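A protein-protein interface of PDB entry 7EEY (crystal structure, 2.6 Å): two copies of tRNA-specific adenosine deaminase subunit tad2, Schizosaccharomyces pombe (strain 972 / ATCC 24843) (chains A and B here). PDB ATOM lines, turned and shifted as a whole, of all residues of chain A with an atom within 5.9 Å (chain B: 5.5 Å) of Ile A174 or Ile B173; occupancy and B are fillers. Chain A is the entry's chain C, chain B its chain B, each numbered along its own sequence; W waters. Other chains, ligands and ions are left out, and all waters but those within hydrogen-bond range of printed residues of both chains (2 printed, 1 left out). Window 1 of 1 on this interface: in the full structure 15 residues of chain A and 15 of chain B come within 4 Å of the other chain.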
ATOM      1  N   LYS A 119     -12.953  -5.284  24.215  1.00  0.00           N
ATOM      2  CA  LYS A 119     -13.190  -4.073  24.996  1.00  0.00           C
ATOM      3  C   LYS A 119     -12.729  -2.847  24.222  1.00  0.00           C
ATOM      4  O   LYS A 119     -11.554  -2.745  23.845  1.00  0.00           O
ATOM      5  CB  LYS A 119     -12.474  -4.161  26.349  1.00  0.00           C
ATOM      6  CG  LYS A 119     -12.960  -5.307  27.228  1.00  0.00           C
ATOM      7  CD  LYS A 119     -12.288  -5.307  28.590  1.00  0.00           C
ATOM      8  CE  LYS A 119     -10.796  -5.585  28.481  1.00  0.00           C
ATOM      9  NZ  LYS A 119     -10.474  -6.595  27.436  1.00  0.00           N
ATOM     10  N   ILE A 120     -13.654  -1.911  24.017  1.00  0.00           N
ATOM     11  CA  ILE A 120     -13.437  -0.700  23.239  1.00  0.00           C
ATOM     12  C   ILE A 120     -13.784   0.503  24.103  1.00  0.00           C
ATOM     13  O   ILE A 120     -14.765   0.477  24.854  1.00  0.00           O
ATOM     14  CB  ILE A 120     -14.291  -0.711  21.953  1.00  0.00           C
ATOM     15  CG1 ILE A 120     -13.949  -1.931  21.096  1.00  0.00           C
ATOM     16  CG2 ILE A 120     -14.103   0.572  21.161  1.00  0.00           C
ATOM     17  CD1 ILE A 120     -14.984  -2.243  20.038  1.00  0.00           C
ATOM     18  N   PHE A 121     -12.973   1.554  24.005  1.00  0.00           N
ATOM     19  CA  PHE A 121     -13.285   2.848  24.600  1.00  0.00           C
ATOM     20  C   PHE A 121     -13.308   3.893  23.495  1.00  0.00           C
ATOM     21  O   PHE A 121     -12.288   4.126  22.837  1.00  0.00           O
ATOM     22  CB  PHE A 121     -12.274   3.233  25.683  1.00  0.00           C
ATOM     23  CG  PHE A 121     -12.667   4.458  26.467  1.00  0.00           C
ATOM     24  CD1 PHE A 121     -13.347   4.340  27.669  1.00  0.00           C
ATOM     25  CD2 PHE A 121     -12.359   5.729  26.002  1.00  0.00           C
ATOM     26  CE1 PHE A 121     -13.711   5.462  28.392  1.00  0.00           C
ATOM     27  CE2 PHE A 121     -12.722   6.856  26.718  1.00  0.00           C
ATOM     28  CZ  PHE A 121     -13.398   6.722  27.916  1.00  0.00           C
ATOM     29  N   VAL A 122     -14.464   4.519  23.296  1.00  0.00           N
ATOM     30  CA  VAL A 122     -14.608   5.589  22.314  1.00  0.00           C
ATOM     31  C   VAL A 122     -14.112   6.877  22.964  1.00  0.00           C
ATOM     32  O   VAL A 122     -14.798   7.459  23.807  1.00  0.00           O
ATOM     33  CB  VAL A 122     -16.059   5.729  21.843  1.00  0.00           C
ATOM     34  CG1 VAL A 122     -16.183   6.856  20.832  1.00  0.00           C
ATOM     35  CG2 VAL A 122     -16.551   4.420  21.253  1.00  0.00           C
ATOM     36  N   TYR A 123     -12.916   7.320  22.586  1.00  0.00           N
ATOM     37  CA  TYR A 123     -12.274   8.455  23.231  1.00  0.00           C
ATOM     38  C   TYR A 123     -12.556   9.730  22.450  1.00  0.00           C
ATOM     39  O   TYR A 123     -12.425   9.759  21.221  1.00  0.00           O
ATOM     40  CB  TYR A 123     -10.765   8.239  23.354  1.00  0.00           C
ATOM     41  CG  TYR A 123     -10.049   9.334  24.119  1.00  0.00           C
ATOM     42  CD1 TYR A 123      -9.756   9.185  25.467  1.00  0.00           C
ATOM     43  CD2 TYR A 123      -9.659  10.513  23.491  1.00  0.00           C
ATOM     44  CE1 TYR A 123      -9.102  10.177  26.170  1.00  0.00           C
ATOM     45  CE2 TYR A 123      -9.008  11.512  24.185  1.00  0.00           C
ATOM     46  CZ  TYR A 123      -8.730  11.340  25.523  1.00  0.00           C
ATOM     47  OH  TYR A 123      -8.078  12.333  26.216  1.00  0.00           O
ATOM     48  N   ARG A 168     -10.532   4.155  30.940  1.00  0.00           N
ATOM     49  CA  ARG A 168     -10.350   4.118  29.491  1.00  0.00           C
ATOM     50  C   ARG A 168      -9.219   3.181  29.077  1.00  0.00           C
ATOM     51  O   ARG A 168      -9.310   2.533  28.027  1.00  0.00           O
ATOM     52  CB  ARG A 168     -10.117   5.530  28.944  1.00  0.00           C
ATOM     53  CG  ARG A 168      -8.697   6.046  29.050  1.00  0.00           C
ATOM     54  CD  ARG A 168      -8.659   7.554  28.883  1.00  0.00           C
ATOM     55  NE  ARG A 168      -7.330   8.091  29.147  1.00  0.00           N
ATOM     56  CZ  ARG A 168      -6.838   8.297  30.364  1.00  0.00           C
ATOM     57  NH1 ARG A 168      -7.564   8.008  31.437  1.00  0.00           N
ATOM     58  NH2 ARG A 168      -5.617   8.789  30.509  1.00  0.00           N
ATOM     59  N   GLU A 169      -8.167   3.066  29.886  1.00  0.00           N
ATOM     60  CA  GLU A 169      -7.040   2.217  29.517  1.00  0.00           C
ATOM     61  C   GLU A 169      -7.274   0.743  29.825  1.00  0.00           C
ATOM     62  O   GLU A 169      -6.358  -0.064  29.630  1.00  0.00           O
ATOM     63  CB  GLU A 169      -5.760   2.709  30.199  1.00  0.00           C
ATOM     64  CG  GLU A 169      -5.189   3.963  29.548  1.00  0.00           C
ATOM     65  CD  GLU A 169      -4.083   4.606  30.360  1.00  0.00           C
ATOM     66  OE1 GLU A 169      -3.086   3.916  30.660  1.00  0.00           O
ATOM     67  OE2 GLU A 169      -4.210   5.802  30.696  1.00  0.00           O
ATOM     68  N   ALA A 171      -9.506  -0.753  28.037  1.00  0.00           N
ATOM     69  CA  ALA A 171      -9.942  -1.214  26.730  1.00  0.00           C
ATOM     70  C   ALA A 171      -8.829  -1.976  26.023  1.00  0.00           C
ATOM     71  O   ALA A 171      -7.641  -1.752  26.264  1.00  0.00           O
ATOM     72  CB  ALA A 171     -10.382  -0.030  25.868  1.00  0.00           C
ATOM     73  N   ASP A 172      -9.227  -2.906  25.155  1.00  0.00           N
ATOM     74  CA  ASP A 172      -8.276  -3.450  24.194  1.00  0.00           C
ATOM     75  C   ASP A 172      -8.007  -2.441  23.088  1.00  0.00           C
ATOM     76  O   ASP A 172      -6.872  -2.316  22.612  1.00  0.00           O
ATOM     77  CB  ASP A 172      -8.799  -4.757  23.599  1.00  0.00           C
ATOM     78  CG  ASP A 172      -9.155  -5.782  24.653  1.00  0.00           C
ATOM     79  OD1 ASP A 172     -10.357  -6.088  24.798  1.00  0.00           O
ATOM     80  OD2 ASP A 172      -8.236  -6.290  25.329  1.00  0.00           O
ATOM     81  N   ILE A 173      -9.038  -1.706  22.678  1.00  0.00           N
ATOM     82  CA  ILE A 173      -8.940  -0.740  21.592  1.00  0.00           C
ATOM     83  C   ILE A 173      -9.482   0.596  22.076  1.00  0.00           C
ATOM     84  O   ILE A 173     -10.621   0.672  22.550  1.00  0.00           O
ATOM     85  CB  ILE A 173      -9.718  -1.203  20.347  1.00  0.00           C
ATOM     86  CG1 ILE A 173      -9.130  -2.498  19.791  1.00  0.00           C
ATOM     87  CG2 ILE A 173      -9.726  -0.112  19.288  1.00  0.00           C
ATOM     88  CD1 ILE A 173      -9.970  -3.108  18.692  1.00  0.00           C
ATOM     89  N   ILE A 174      -8.680   1.645  21.943  1.00  0.00           N
ATOM     90  CA  ILE A 174      -9.151   3.009  22.146  1.00  0.00           C
ATOM     91  C   ILE A 174      -9.346   3.638  20.776  1.00  0.00           C
ATOM     92  O   ILE A 174      -8.424   3.655  19.950  1.00  0.00           O
ATOM     93  CB  ILE A 174      -8.183   3.825  23.014  1.00  0.00           C
ATOM     94  CG1 ILE A 174      -8.200   3.286  24.445  1.00  0.00           C
ATOM     95  CG2 ILE A 174      -8.573   5.294  22.999  1.00  0.00           C
ATOM     96  CD1 ILE A 174      -7.301   4.033  25.394  1.00  0.00           C
ATOM     97  N   LEU A 175     -10.557   4.130  20.525  1.00  0.00           N
ATOM     98  CA  LEU A 175     -10.934   4.676  19.227  1.00  0.00           C
ATOM     99  C   LEU A 175     -11.030   6.190  19.333  1.00  0.00           C
ATOM    100  O   LEU A 175     -12.005   6.711  19.899  1.00  0.00           O
ATOM    101  CB  LEU A 175     -12.265   4.084  18.754  1.00  0.00           C
ATOM    102  CG  LEU A 175     -12.573   4.158  17.253  1.00  0.00           C
ATOM    103  CD1 LEU A 175     -13.589   3.103  16.868  1.00  0.00           C
ATOM    104  CD2 LEU A 175     -13.075   5.533  16.841  1.00  0.00           C
ATOM    105  N   PRO A 176     -10.056   6.936  18.817  1.00  0.00           N
ATOM    106  CA  PRO A 176     -10.159   8.399  18.848  1.00  0.00           C
ATOM    107  C   PRO A 176     -11.247   8.865  17.894  1.00  0.00           C
ATOM    108  O   PRO A 176     -11.263   8.494  16.718  1.00  0.00           O
ATOM    109  CB  PRO A 176      -8.769   8.873  18.403  1.00  0.00           C
ATOM    110  CG  PRO A 176      -7.944   7.626  18.193  1.00  0.00           C
ATOM    111  CD  PRO A 176      -8.880   6.479  18.065  1.00  0.00           C
ATOM    112  N   THR A 183     -11.761   4.500   8.712  1.00  0.00           N
ATOM    113  CA  THR A 183     -10.654   3.555   8.844  1.00  0.00           C
ATOM    114  C   THR A 183     -10.748   2.785  10.157  1.00  0.00           C
ATOM    115  O   THR A 183     -10.571   1.559  10.191  1.00  0.00           O
ATOM    116  CB  THR A 183      -9.316   4.291   8.742  1.00  0.00           C
ATOM    117  OG1 THR A 183      -9.347   5.195   7.632  1.00  0.00           O
ATOM    118  CG2 THR A 183      -8.173   3.302   8.551  1.00  0.00           C
ATOM    119  N   ALA A 184     -11.044   3.489  11.253  1.00  0.00           N
ATOM    120  CA  ALA A 184     -11.192   2.819  12.541  1.00  0.00           C
ATOM    121  C   ALA A 184     -12.430   1.929  12.561  1.00  0.00           C
ATOM    122  O   ALA A 184     -12.408   0.836  13.141  1.00  0.00           O
ATOM    123  CB  ALA A 184     -11.248   3.853  13.665  1.00  0.00           C
ATOM    124  N   PHE A 187     -11.403  -1.193  10.834  1.00  0.00           N
ATOM    125  CA  PHE A 187     -10.557  -1.986  11.725  1.00  0.00           C
ATOM    126  C   PHE A 187     -11.401  -2.767  12.732  1.00  0.00           C
ATOM    127  O   PHE A 187     -11.209  -3.977  12.923  1.00  0.00           O
ATOM    128  CB  PHE A 187      -9.557  -1.063  12.433  1.00  0.00           C
ATOM    129  CG  PHE A 187      -8.599  -1.770  13.358  1.00  0.00           C
ATOM    130  CD1 PHE A 187      -7.327  -2.114  12.927  1.00  0.00           C
ATOM    131  CD2 PHE A 187      -8.953  -2.051  14.670  1.00  0.00           C
ATOM    132  CE1 PHE A 187      -6.438  -2.750  13.776  1.00  0.00           C
ATOM    133  CE2 PHE A 187      -8.067  -2.688  15.524  1.00  0.00           C
ATOM    134  CZ  PHE A 187      -6.808  -3.036  15.075  1.00  0.00           C
ATOM    135  N   VAL A 188     -12.364  -2.095  13.365  1.00  0.00           N
ATOM    136  CA  VAL A 188     -13.149  -2.746  14.412  1.00  0.00           C
ATOM    137  C   VAL A 188     -14.087  -3.793  13.817  1.00  0.00           C
ATOM    138  O   VAL A 188     -14.298  -4.863  14.405  1.00  0.00           O
ATOM    139  CB  VAL A 188     -13.910  -1.700  15.246  1.00  0.00           C
ATOM    140  CG1 VAL A 188     -14.703  -2.377  16.353  1.00  0.00           C
ATOM    141  CG2 VAL A 188     -12.939  -0.696  15.842  1.00  0.00           C
ATOM    142  N   LYS B 119      -3.051   3.864  10.545  1.00  0.00           N
ATOM    143  CA  LYS B 119      -2.396   4.713  11.535  1.00  0.00           C
ATOM    144  C   LYS B 119      -2.728   4.204  12.932  1.00  0.00           C
ATOM    145  O   LYS B 119      -3.900   4.192  13.342  1.00  0.00           O
ATOM    146  CB  LYS B 119      -2.818   6.173  11.369  1.00  0.00           C
ATOM    147  CG  LYS B 119      -2.571   6.711   9.971  1.00  0.00           C
ATOM    148  CD  LYS B 119      -2.897   8.183   9.873  1.00  0.00           C
ATOM    149  CE  LYS B 119      -4.395   8.416   9.940  1.00  0.00           C
ATOM    150  NZ  LYS B 119      -5.131   7.528   9.000  1.00  0.00           N
ATOM    151  N   ILE B 120      -1.691   3.795  13.660  1.00  0.00           N
ATOM    152  CA  ILE B 120      -1.832   3.177  14.969  1.00  0.00           C
ATOM    153  C   ILE B 120      -0.907   3.895  15.938  1.00  0.00           C
ATOM    154  O   ILE B 120       0.215   4.267  15.580  1.00  0.00           O
ATOM    155  CB  ILE B 120      -1.513   1.667  14.905  1.00  0.00           C
ATOM    156  CG1 ILE B 120      -2.522   0.957  14.000  1.00  0.00           C
ATOM    157  CG2 ILE B 120      -1.504   1.042  16.294  1.00  0.00           C
ATOM    158  CD1 ILE B 120      -2.057  -0.389  13.500  1.00  0.00           C
ATOM    159  N   PHE B 121      -1.395   4.122  17.155  1.00  0.00           N
ATOM    160  CA  PHE B 121      -0.582   4.655  18.240  1.00  0.00           C
ATOM    161  C   PHE B 121      -0.562   3.637  19.370  1.00  0.00           C
ATOM    162  O   PHE B 121      -1.615   3.285  19.910  1.00  0.00           O
ATOM    163  CB  PHE B 121      -1.116   5.998  18.743  1.00  0.00           C
ATOM    164  CG  PHE B 121      -0.174   6.709  19.675  1.00  0.00           C
ATOM    165  CD1 PHE B 121       0.719   7.646  19.187  1.00  0.00           C
ATOM    166  CD2 PHE B 121      -0.173   6.431  21.032  1.00  0.00           C
ATOM    167  CE1 PHE B 121       1.591   8.300  20.037  1.00  0.00           C
ATOM    168  CE2 PHE B 121       0.697   7.080  21.886  1.00  0.00           C
ATOM    169  CZ  PHE B 121       1.580   8.016  21.387  1.00  0.00           C
ATOM    170  N   ALA B 171      -4.116   9.100  15.196  1.00  0.00           N
ATOM    171  CA  ALA B 171      -4.167   7.699  14.817  1.00  0.00           C
ATOM    172  C   ALA B 171      -5.598   7.280  14.521  1.00  0.00           C
ATOM    173  O   ALA B 171      -6.559   7.842  15.054  1.00  0.00           O
ATOM    174  CB  ALA B 171      -3.589   6.820  15.927  1.00  0.00           C
ATOM    175  N   ASP B 172      -5.738   6.296  13.635  1.00  0.00           N
ATOM    176  CA  ASP B 172      -7.024   5.627  13.511  1.00  0.00           C
ATOM    177  C   ASP B 172      -7.302   4.786  14.745  1.00  0.00           C
ATOM    178  O   ASP B 172      -8.406   4.832  15.299  1.00  0.00           O
ATOM    179  CB  ASP B 172      -7.061   4.756  12.257  1.00  0.00           C
ATOM    180  CG  ASP B 172      -6.868   5.553  10.991  1.00  0.00           C
ATOM    181  OD1 ASP B 172      -5.893   5.275  10.261  1.00  0.00           O
ATOM    182  OD2 ASP B 172      -7.690   6.455  10.728  1.00  0.00           O
ATOM    183  N   ILE B 173      -6.309   4.026  15.203  1.00  0.00           N
ATOM    184  CA  ILE B 173      -6.508   3.128  16.333  1.00  0.00           C
ATOM    185  C   ILE B 173      -5.424   3.374  17.373  1.00  0.00           C
ATOM    186  O   ILE B 173      -4.231   3.409  17.045  1.00  0.00           O
ATOM    187  CB  ILE B 173      -6.524   1.652  15.893  1.00  0.00           C
ATOM    188  CG1 ILE B 173      -7.774   1.363  15.056  1.00  0.00           C
ATOM    189  CG2 ILE B 173      -6.482   0.735  17.100  1.00  0.00           C
ATOM    190  CD1 ILE B 173      -9.076   1.518  15.818  1.00  0.00           C
ATOM    191  N   ILE B 174      -5.843   3.556  18.623  1.00  0.00           N
ATOM    192  CA  ILE B 174      -4.944   3.648  19.765  1.00  0.00           C
ATOM    193  C   ILE B 174      -5.017   2.327  20.518  1.00  0.00           C
ATOM    194  O   ILE B 174      -6.095   1.913  20.961  1.00  0.00           O
ATOM    195  CB  ILE B 174      -5.312   4.826  20.682  1.00  0.00           C
ATOM    196  CG1 ILE B 174      -5.038   6.160  19.987  1.00  0.00           C
ATOM    197  CG2 ILE B 174      -4.546   4.742  21.993  1.00  0.00           C
ATOM    198  CD1 ILE B 174      -5.567   7.360  20.750  1.00  0.00           C
ATOM    199  N   LEU B 175      -3.875   1.661  20.655  1.00  0.00           N
ATOM    200  CA  LEU B 175      -3.810   0.393  21.370  1.00  0.00           C
ATOM    201  C   LEU B 175      -3.200   0.620  22.745  1.00  0.00           C
ATOM    202  O   LEU B 175      -1.985   0.849  22.857  1.00  0.00           O
ATOM    203  CB  LEU B 175      -3.001  -0.636  20.576  1.00  0.00           C
ATOM    204  CG  LEU B 175      -3.632  -1.023  19.237  1.00  0.00           C
ATOM    205  CD1 LEU B 175      -2.746  -1.996  18.481  1.00  0.00           C
ATOM    206  CD2 LEU B 175      -5.024  -1.608  19.445  1.00  0.00           C
ATOM    207  N   PRO B 176      -3.998   0.618  23.811  1.00  0.00           N
ATOM    208  CA  PRO B 176      -3.429   0.761  25.153  1.00  0.00           C
ATOM    209  C   PRO B 176      -2.717  -0.510  25.573  1.00  0.00           C
ATOM    210  O   PRO B 176      -3.188  -1.626  25.336  1.00  0.00           O
ATOM    211  CB  PRO B 176      -4.647   1.041  26.040  1.00  0.00           C
ATOM    212  CG  PRO B 176      -5.810   0.540  25.279  1.00  0.00           C
ATOM    213  CD  PRO B 176      -5.462   0.470  23.827  1.00  0.00           C
HETATM  214  O   HOH W   1     -10.422   6.463  11.315  1.00  0.00           O
HETATM  215  O   HOH W   2     -10.144   7.020  14.646  1.00  0.00           O
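O of Ala A171 touches CG of Pro B176 (3.1 Å).
Asp A172 touches Pro B176 (O to CD, 3.4 Å).
Ile B173 touches Ile A173 (CD1 to CG2, 3.9 Å).
Ile A173 touches Ile B174.
C of Ile B173 touches O of Ile A174, 3.96 Å away.
Ile A174 touches Pro B176.
CB of Thr A183 touches OD2 of Asp B172, at 3.4 Å.
CB of Ala A184 touches O of Asp B172 (3.4 Å).
Ala A184 touches Ile B173 (CB to CD1, 3.8 Å).
Ile B173 touches Phe A187.
Printed residues of chain B that touch a printed residue of chain A: Ala B171, Asp B172, Ile B173, Ile B174, Leu B175 and Pro B176.
Hydrophobic or aromatic side chains of chain B that line the printed part of chain A: Ile B173, Ile B174, Leu B175 and Pro B176.
Printed residues of chain A that touch a printed residue of chain B: Ala A171, Asp A172, Ile A173, Ile A174, Pro A176, Thr A183, Ala A184 and Phe A187.
Among the printed residues, 15 pairs touch across the chains.
Among the printed residues, no Asp or Glu carboxylate lies within 4 Å of a Lys or Arg side-chain nitrogen of the other chain.
NZ of Lys B119 lies within salt-bridge range of OD1 of Asp B172 (2.7 Å).
The backbone NH (N) of Ile B173 is in hydrogen-bond range of the backbone carbonyl oxygen (O) of Lys B119 (3.0 Å).
The backbone NH of Phe B121 sits at hydrogen-bond distance from the backbone carbonyl oxygen of Ile B173, at 2.9 Å.
The backbone NH (N) of Leu B175 sits at hydrogen-bond distance from the backbone carbonyl oxygen (O) of Phe B121 (2.9 Å).
The side-chain amino group of Lys A119 is in salt-bridge range of the side-chain carboxylate of Asp A172.
The backbone carbonyl oxygen (O) of Lys A119 is in hydrogen-bond range of the backbone NH (N) of Ile A173, 3.0 Å away.
Ile A174 touches just these residues of chain B: Ile B173 (3.96 Å), Ile B174 (2.8 Å) and Pro B176 (3.7 Å).
Of chain A, only Ile A173, Ile A174, Ala A184 and Phe A187 come within 4 Å of Ile B173.
Printed residues of chain B within 4 Å of Ala A171: Pro B176.
Of the printed residues of chain A, Ala B171 touches Pro A176 (3.4 Å).
Of the printed residues of chain A, Leu B175 touches Asp A172 (3.7 Å).
The nearest printed residue of chain A that does not touch Ala B171 is Ala A184 (6.3 Å).
Water W2 lies within hydrogen-bond range of O of Pro A176 and O of Asp B172.
Water W1 lies within hydrogen-bond range of the side-chain carboxylate of Asp B172 (2.8 Å) and the backbone NH of Ala A184 (3.0 Å).
N of Ile A174 sits at hydrogen-bond distance from O of Ile B174, 2.8 Å away.
Asp A172 touches Leu B175, but with the chains exchanged Leu A175 does not touch Asp B172 (4.7 Å).
Ile B173 touches its own counterpart, Ile A173.
Ile A173 touches Ile B174, and with the chains exchanged Ile A174 touches Ile B173.
Ile A174 touches Pro B176, and with the chains exchanged Pro A176 touches Ile B174.
9 positions are printed for both chains.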
